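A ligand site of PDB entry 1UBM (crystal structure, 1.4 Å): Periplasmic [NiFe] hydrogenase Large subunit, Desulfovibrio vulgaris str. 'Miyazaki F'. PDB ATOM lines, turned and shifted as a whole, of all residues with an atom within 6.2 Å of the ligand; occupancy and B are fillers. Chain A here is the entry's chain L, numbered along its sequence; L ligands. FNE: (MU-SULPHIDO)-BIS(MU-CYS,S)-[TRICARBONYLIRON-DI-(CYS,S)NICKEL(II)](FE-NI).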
ATOM      1  N   GLU A  16      21.229  26.066 -18.967  1.00  0.00           N
ATOM      2  CA  GLU A  16      20.322  26.980 -18.312  1.00  0.00           C
ATOM      3  C   GLU A  16      21.033  28.349 -18.332  1.00  0.00           C
ATOM      4  O   GLU A  16      22.150  28.536 -17.901  1.00  0.00           O
ATOM      5  CB  GLU A  16      19.912  26.533 -16.912  1.00  0.00           C
ATOM      6  CG  GLU A  16      18.785  27.272 -16.228  1.00  0.00           C
ATOM      7  CD  GLU A  16      19.002  28.740 -15.893  1.00  0.00           C
ATOM      8  OE1 GLU A  16      18.209  29.692 -15.997  1.00  0.00           O
ATOM      9  OE2 GLU A  16      20.245  28.998 -15.661  1.00  0.00           O
ATOM     10  N   THR A  62      16.255  30.607  -7.611  1.00  0.00           N
ATOM     11  CA  THR A  62      17.530  30.802  -8.277  1.00  0.00           C
ATOM     12  C   THR A  62      17.566  30.023  -9.598  1.00  0.00           C
ATOM     13  O   THR A  62      18.106  30.474 -10.607  1.00  0.00           O
ATOM     14  CB  THR A  62      18.674  30.271  -7.409  1.00  0.00           C
ATOM     15  OG1 THR A  62      18.790  31.062  -6.209  1.00  0.00           O
ATOM     16  CG2 THR A  62      19.993  30.369  -8.151  1.00  0.00           C
ATOM     17  N   CYS A  63      16.930  28.849  -9.541  1.00  0.00           N
ATOM     18  CA  CYS A  63      17.009  27.936 -10.679  1.00  0.00           C
ATOM     19  C   CYS A  63      15.908  26.897 -10.671  1.00  0.00           C
ATOM     20  O   CYS A  63      15.679  26.231  -9.650  1.00  0.00           O
ATOM     21  CB  CYS A  63      18.376  27.223 -10.698  1.00  0.00           C
ATOM     22  SG  CYS A  63      18.556  26.225 -12.211  1.00  0.00           S
ATOM     23  N   GLY A  64      15.269  26.752 -11.826  1.00  0.00           N
ATOM     24  CA  GLY A  64      14.197  25.767 -11.983  1.00  0.00           C
ATOM     25  C   GLY A  64      14.587  24.486 -12.680  1.00  0.00           C
ATOM     26  O   GLY A  64      13.748  23.572 -12.808  1.00  0.00           O
ATOM     27  N   VAL A  65      15.837  24.451 -13.128  1.00  0.00           N
ATOM     28  CA  VAL A  65      16.469  23.234 -13.675  1.00  0.00           C
ATOM     29  C   VAL A  65      16.935  22.458 -12.452  1.00  0.00           C
ATOM     30  O   VAL A  65      16.401  21.349 -12.234  1.00  0.00           O
ATOM     31  CB  VAL A  65      17.610  23.513 -14.662  1.00  0.00           C
ATOM     32  CG1 VAL A  65      18.333  22.232 -15.066  1.00  0.00           C
ATOM     33  CG2 VAL A  65      17.073  24.261 -15.886  1.00  0.00           C
ATOM     34  N   CYS A  66      17.832  23.007 -11.639  1.00  0.00           N
ATOM     35  CA  CYS A  66      18.164  22.374 -10.354  1.00  0.00           C
ATOM     36  C   CYS A  66      17.183  22.888  -9.309  1.00  0.00           C
ATOM     37  O   CYS A  66      17.477  23.417  -8.240  1.00  0.00           O
ATOM     38  CB  CYS A  66      19.635  22.634 -10.015  1.00  0.00           C
ATOM     39  SG  CYS A  66      20.031  24.374  -9.726  1.00  0.00           S
ATOM     40  N   THR A  67      15.912  22.759  -9.664  1.00  0.00           N
ATOM     41  CA  THR A  67      14.841  23.011  -8.721  1.00  0.00           C
ATOM     42  C   THR A  67      15.123  22.105  -7.543  1.00  0.00           C
ATOM     43  O   THR A  67      15.829  21.110  -7.514  1.00  0.00           O
ATOM     44  CB  THR A  67      13.504  22.719  -9.405  1.00  0.00           C
ATOM     45  OG1 THR A  67      12.506  22.974  -8.435  1.00  0.00           O
ATOM     46  CG2 THR A  67      13.200  21.256  -9.702  1.00  0.00           C
ATOM     47  N   THR A  69      17.019  22.067  -5.115  1.00  0.00           N
ATOM     48  CA  THR A  69      18.320  22.114  -4.481  1.00  0.00           C
ATOM     49  C   THR A  69      18.544  23.354  -3.612  1.00  0.00           C
ATOM     50  O   THR A  69      19.096  23.228  -2.520  1.00  0.00           O
ATOM     51  CB  THR A  69      19.478  22.016  -5.480  1.00  0.00           C
ATOM     52  OG1 THR A  69      19.472  23.166  -6.347  1.00  0.00           O
ATOM     53  CG2 THR A  69      19.317  20.734  -6.301  1.00  0.00           C
ATOM     54  N   HIS A  70      18.114  24.507  -4.119  1.00  0.00           N
ATOM     55  CA  HIS A  70      18.304  25.721  -3.315  1.00  0.00           C
ATOM     56  C   HIS A  70      17.340  25.814  -2.126  1.00  0.00           C
ATOM     57  O   HIS A  70      17.674  26.336  -1.072  1.00  0.00           O
ATOM     58  CB  HIS A  70      18.166  26.950  -4.207  1.00  0.00           C
ATOM     59  CG  HIS A  70      19.288  27.093  -5.181  1.00  0.00           C
ATOM     60  ND1 HIS A  70      20.501  27.624  -4.835  1.00  0.00           N
ATOM     61  CD2 HIS A  70      19.358  26.760  -6.490  1.00  0.00           C
ATOM     62  CE1 HIS A  70      21.273  27.603  -5.912  1.00  0.00           C
ATOM     63  NE2 HIS A  70      20.620  27.086  -6.952  1.00  0.00           N
ATOM     64  N   ASP A 105      17.560  15.285 -13.568  1.00  0.00           N
ATOM     65  CA  ASP A 105      18.462  16.305 -14.078  1.00  0.00           C
ATOM     66  C   ASP A 105      19.500  15.729 -15.029  1.00  0.00           C
ATOM     67  O   ASP A 105      19.678  16.187 -16.173  1.00  0.00           O
ATOM     68  CB  ASP A 105      19.060  17.042 -12.864  1.00  0.00           C
ATOM     69  CG  ASP A 105      19.638  18.407 -13.183  1.00  0.00           C
ATOM     70  OD1 ASP A 105      20.085  18.676 -14.337  1.00  0.00           O
ATOM     71  OD2 ASP A 105      19.704  19.237 -12.248  1.00  0.00           O
ATOM     72  N   ALA A 459      24.690  19.354  -5.240  1.00  0.00           N
ATOM     73  CA  ALA A 459      23.651  19.376  -6.267  1.00  0.00           C
ATOM     74  C   ALA A 459      24.115  18.650  -7.506  1.00  0.00           C
ATOM     75  O   ALA A 459      25.299  18.282  -7.590  1.00  0.00           O
ATOM     76  CB  ALA A 459      23.318  20.833  -6.582  1.00  0.00           C
ATOM     77  N   PRO A 460      23.297  18.402  -8.495  1.00  0.00           N
ATOM     78  CA  PRO A 460      23.782  17.735  -9.723  1.00  0.00           C
ATOM     79  C   PRO A 460      24.991  18.411 -10.382  1.00  0.00           C
ATOM     80  O   PRO A 460      25.758  17.690 -11.057  1.00  0.00           O
ATOM     81  CB  PRO A 460      22.540  17.737 -10.637  1.00  0.00           C
ATOM     82  CG  PRO A 460      21.389  17.749  -9.668  1.00  0.00           C
ATOM     83  CD  PRO A 460      21.843  18.637  -8.523  1.00  0.00           C
ATOM     84  N   ARG A 461      25.206  19.727 -10.193  1.00  0.00           N
ATOM     85  CA  ARG A 461      26.378  20.373 -10.805  1.00  0.00           C
ATOM     86  C   ARG A 461      27.507  20.624  -9.817  1.00  0.00           C
ATOM     87  O   ARG A 461      28.548  21.176 -10.163  1.00  0.00           O
ATOM     88  CB  ARG A 461      25.955  21.669 -11.497  1.00  0.00           C
ATOM     89  CG  ARG A 461      25.033  21.413 -12.676  1.00  0.00           C
ATOM     90  CD  ARG A 461      24.218  22.642 -13.108  1.00  0.00           C
ATOM     91  NE  ARG A 461      23.342  22.156 -14.176  1.00  0.00           N
ATOM     92  CZ  ARG A 461      22.269  21.433 -13.978  1.00  0.00           C
ATOM     93  NH1 ARG A 461      21.825  21.080 -12.771  1.00  0.00           N
ATOM     94  NH2 ARG A 461      21.576  21.042 -15.028  1.00  0.00           N
ATOM     95  N   GLY A 462      27.318  20.202  -8.551  1.00  0.00           N
ATOM     96  CA  GLY A 462      28.346  20.257  -7.547  1.00  0.00           C
ATOM     97  C   GLY A 462      28.046  20.959  -6.264  1.00  0.00           C
ATOM     98  O   GLY A 462      26.906  21.054  -5.821  1.00  0.00           O
ATOM     99  N   GLY A 463      29.064  21.461  -5.572  1.00  0.00           N
ATOM    100  CA  GLY A 463      28.979  21.946  -4.208  1.00  0.00           C
ATOM    101  C   GLY A 463      28.273  23.287  -4.132  1.00  0.00           C
ATOM    102  O   GLY A 463      28.802  24.312  -4.532  1.00  0.00           O
ATOM    103  N   LEU A 464      27.082  23.229  -3.544  1.00  0.00           N
ATOM    104  CA  LEU A 464      26.238  24.382  -3.293  1.00  0.00           C
ATOM    105  C   LEU A 464      26.271  24.746  -1.810  1.00  0.00           C
ATOM    106  O   LEU A 464      26.106  23.854  -0.977  1.00  0.00           O
ATOM    107  CB  LEU A 464      24.809  24.058  -3.721  1.00  0.00           C
ATOM    108  CG  LEU A 464      23.715  25.014  -3.289  1.00  0.00           C
ATOM    109  CD1 LEU A 464      23.940  26.381  -3.911  1.00  0.00           C
ATOM    110  CD2 LEU A 464      22.330  24.471  -3.655  1.00  0.00           C
ATOM    111  N   VAL A 482      27.402  28.952  -5.625  1.00  0.00           N
ATOM    112  CA  VAL A 482      26.688  27.896  -6.346  1.00  0.00           C
ATOM    113  C   VAL A 482      27.648  27.106  -7.245  1.00  0.00           C
ATOM    114  O   VAL A 482      28.655  27.690  -7.643  1.00  0.00           O
ATOM    115  CB  VAL A 482      25.552  28.572  -7.122  1.00  0.00           C
ATOM    116  CG1 VAL A 482      24.547  27.641  -7.723  1.00  0.00           C
ATOM    117  CG2 VAL A 482      24.727  29.441  -6.175  1.00  0.00           C
ATOM    118  N   PRO A 483      27.418  25.818  -7.509  1.00  0.00           N
ATOM    119  CA  PRO A 483      28.364  25.028  -8.315  1.00  0.00           C
ATOM    120  C   PRO A 483      28.785  25.727  -9.609  1.00  0.00           C
ATOM    121  O   PRO A 483      30.001  25.791  -9.848  1.00  0.00           O
ATOM    122  CB  PRO A 483      27.640  23.729  -8.617  1.00  0.00           C
ATOM    123  CG  PRO A 483      26.375  23.755  -7.841  1.00  0.00           C
ATOM    124  CD  PRO A 483      26.315  24.970  -7.018  1.00  0.00           C
ATOM    125  N   SER A 484      27.876  26.241 -10.416  1.00  0.00           N
ATOM    126  CA  SER A 484      28.320  26.886 -11.652  1.00  0.00           C
ATOM    127  C   SER A 484      29.130  28.166 -11.412  1.00  0.00           C
ATOM    128  O   SER A 484      29.878  28.578 -12.310  1.00  0.00           O
ATOM    129  CB  SER A 484      27.133  27.230 -12.547  1.00  0.00           C
ATOM    130  OG  SER A 484      26.534  26.067 -13.064  1.00  0.00           O
ATOM    131  N   THR A 485      28.983  28.760 -10.215  1.00  0.00           N
ATOM    132  CA  THR A 485      29.830  29.902  -9.863  1.00  0.00           C
ATOM    133  C   THR A 485      31.294  29.449  -9.823  1.00  0.00           C
ATOM    134  O   THR A 485      32.145  30.095 -10.442  1.00  0.00           O
ATOM    135  CB  THR A 485      29.425  30.539  -8.505  1.00  0.00           C
ATOM    136  OG1 THR A 485      28.005  30.584  -8.320  1.00  0.00           O
ATOM    137  CG2 THR A 485      29.930  31.982  -8.463  1.00  0.00           C
ATOM    138  N   ASP A 526      27.813  21.169 -17.724  1.00  0.00           N
ATOM    139  CA  ASP A 526      26.383  21.373 -17.421  1.00  0.00           C
ATOM    140  C   ASP A 526      26.139  22.739 -16.798  1.00  0.00           C
ATOM    141  O   ASP A 526      25.663  22.844 -15.673  1.00  0.00           O
ATOM    142  CB  ASP A 526      25.900  20.261 -16.530  1.00  0.00           C
ATOM    143  CG  ASP A 526      24.447  20.120 -16.239  1.00  0.00           C
ATOM    144  OD1 ASP A 526      24.151  19.240 -15.404  1.00  0.00           O
ATOM    145  OD2 ASP A 526      23.657  20.868 -16.819  1.00  0.00           O
ATOM    146  N   PRO A 527      26.464  23.799 -17.524  1.00  0.00           N
ATOM    147  CA  PRO A 527      26.357  25.152 -16.955  1.00  0.00           C
ATOM    148  C   PRO A 527      24.933  25.547 -16.590  1.00  0.00           C
ATOM    149  O   PRO A 527      23.948  25.264 -17.257  1.00  0.00           O
ATOM    150  CB  PRO A 527      26.840  26.072 -18.093  1.00  0.00           C
ATOM    151  CG  PRO A 527      27.627  25.189 -19.020  1.00  0.00           C
ATOM    152  CD  PRO A 527      26.942  23.854 -18.922  1.00  0.00           C
ATOM    153  N   CYS A 528      24.869  26.295 -15.499  1.00  0.00           N
ATOM    154  CA  CYS A 528      23.601  26.892 -15.092  1.00  0.00           C
ATOM    155  C   CYS A 528      23.854  28.317 -14.657  1.00  0.00           C
ATOM    156  O   CYS A 528      24.406  28.546 -13.600  1.00  0.00           O
ATOM    157  CB  CYS A 528      22.995  26.032 -13.983  1.00  0.00           C
ATOM    158  SG  CYS A 528      21.371  26.590 -13.497  1.00  0.00           S
ATOM    159  N   ILE A 529      23.489  29.282 -15.487  1.00  0.00           N
ATOM    160  CA  ILE A 529      23.940  30.647 -15.222  1.00  0.00           C
ATOM    161  C   ILE A 529      23.066  31.420 -14.251  1.00  0.00           C
ATOM    162  O   ILE A 529      23.500  32.301 -13.496  1.00  0.00           O
ATOM    163  CB  ILE A 529      24.057  31.403 -16.554  1.00  0.00           C
ATOM    164  CG1 ILE A 529      24.835  30.621 -17.612  1.00  0.00           C
ATOM    165  CG2 ILE A 529      24.658  32.767 -16.301  1.00  0.00           C
ATOM    166  CD1 ILE A 529      26.199  30.162 -17.155  1.00  0.00           C
ATOM    167  N   ALA A 530      21.773  31.084 -14.210  1.00  0.00           N
ATOM    168  CA  ALA A 530      20.880  31.591 -13.192  1.00  0.00           C
ATOM    169  C   ALA A 530      21.391  31.198 -11.807  1.00  0.00           C
ATOM    170  O   ALA A 530      21.458  31.943 -10.860  1.00  0.00           O
ATOM    171  CB  ALA A 530      19.485  31.048 -13.414  1.00  0.00           C
ATOM    172  N   CYS A 531      21.779  29.912 -11.726  1.00  0.00           N
ATOM    173  CA  CYS A 531      22.456  29.424 -10.537  1.00  0.00           C
ATOM    174  C   CYS A 531      23.717  30.199 -10.235  1.00  0.00           C
ATOM    175  O   CYS A 531      23.984  30.660  -9.128  1.00  0.00           O
ATOM    176  CB  CYS A 531      22.844  27.935 -10.695  1.00  0.00           C
ATOM    177  SG  CYS A 531      21.591  26.819 -10.036  1.00  0.00           S
ATOM    178  N   GLY A 532      24.565  30.306 -11.248  1.00  0.00           N
ATOM    179  CA  GLY A 532      25.880  30.881 -11.024  1.00  0.00           C
ATOM    180  C   GLY A 532      25.867  32.311 -10.537  1.00  0.00           C
ATOM    181  O   GLY A 532      26.712  32.721  -9.730  1.00  0.00           O
HETATM  182 NI   FNE L   1      20.634  25.398 -11.692  1.00  0.00          NI
HETATM  183 FE   FNE L   1      22.291  24.633  -9.845  1.00  0.00          FE
HETATM  184  C1  FNE L   1      24.004  25.133 -10.313  1.00  0.00           C
HETATM  185  C2  FNE L   1      22.802  22.795  -9.924  1.00  0.00           C
HETATM  186  C3  FNE L   1      22.777  24.637  -8.166  1.00  0.00           C
HETATM  187  O1  FNE L   1      25.077  25.246 -10.859  1.00  0.00           O
HETATM  188  O2  FNE L   1      22.875  21.706  -9.910  1.00  0.00           O
HETATM  189  O3  FNE L   1      23.070  24.532  -7.051  1.00  0.00           O
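The side-chain hydroxyl (OG) of Ser 484 sits at hydrogen-bond distance from the backbone NH (N) of Cys 528 (3.0 Å).
O of Cys 66 lies within hydrogen-bond range of OG1 of Thr 69 (2.8 Å).
The backbone NH of Val 65 lies close to the side-chain sulfur of Cys 63, 3.4 Å away.
The side-chain sulfur of Cys 528 sits close to the side-chain carboxylate of Glu 16, 3.4 Å away.
The side-chain carboxylate (OD2) of Asp 105 is in salt-bridge range of the guanidinium group (NH1) of Arg 461, 2.9 Å away.
The backbone carbonyl oxygen (O) of Val 482 lies within hydrogen-bond range of the side-chain hydroxyl (OG1) of Thr 485, 3.0 Å away.
SG of Cys 531 sits close to NE2 of His 70 (3.2 Å).
The guanidinium group of Arg 461 is in salt-bridge range of the side-chain carboxylate of Asp 526 (2.8 Å).
Thr 69 touches the ligand.
His 70 touches the ligand (NE2 to C3, 3.5 Å).
Ala 459 touches the ligand.
Pro 460 touches the ligand (CD to O2, 3.5 Å).
Leu 464 touches the ligand (CD2 to O3, 3.5 Å).
Val 482 touches the ligand.
CD of Pro 483 touches O3 of the ligand (3.3 Å).
Hydrophobic or aromatic side chains within 4 Å of the ligand: His 70, Ala 459, Pro 460, Leu 464, Val 482 and Pro 483.
13 residues have an atom within 4 Å of the ligand: Cys 63, Cys 66, Thr 69, His 70, Ala 459, Pro 460, Arg 461, Leu 464, Val 482, Pro 483, Ser 484, Cys 528 and Cys 531.
The nearest printed residue that does not touch the ligand is Val 65 (4.6 Å).
The side-chain hydroxyl of Ser 484 is in hydrogen-bond range of an oxygen (O1) of the ligand (2.8 Å).
The side-chain sulfur of Cys 66 binds an iron atom (FE) of the ligand (2.3 Å).
NI of the ligand is bound by SG of Cys 528 (2.3 Å).
The backbone NH (N) of Ser 484 sits at hydrogen-bond distance from an oxygen (O1) of the ligand (3.0 Å).
The side-chain sulfur (SG) of Cys 63 binds a nickel atom (NI) of the ligand (2.3 Å).
An oxygen (O2) of the ligand is in hydrogen-bond range of the guanidinium group (NH1) of Arg 461.
O2 of the ligand lies within hydrogen-bond range of N of Arg 461.
The side-chain sulfur (SG) of Cys 531 is bound to an iron atom (FE) of the ligand (2.3 Å).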
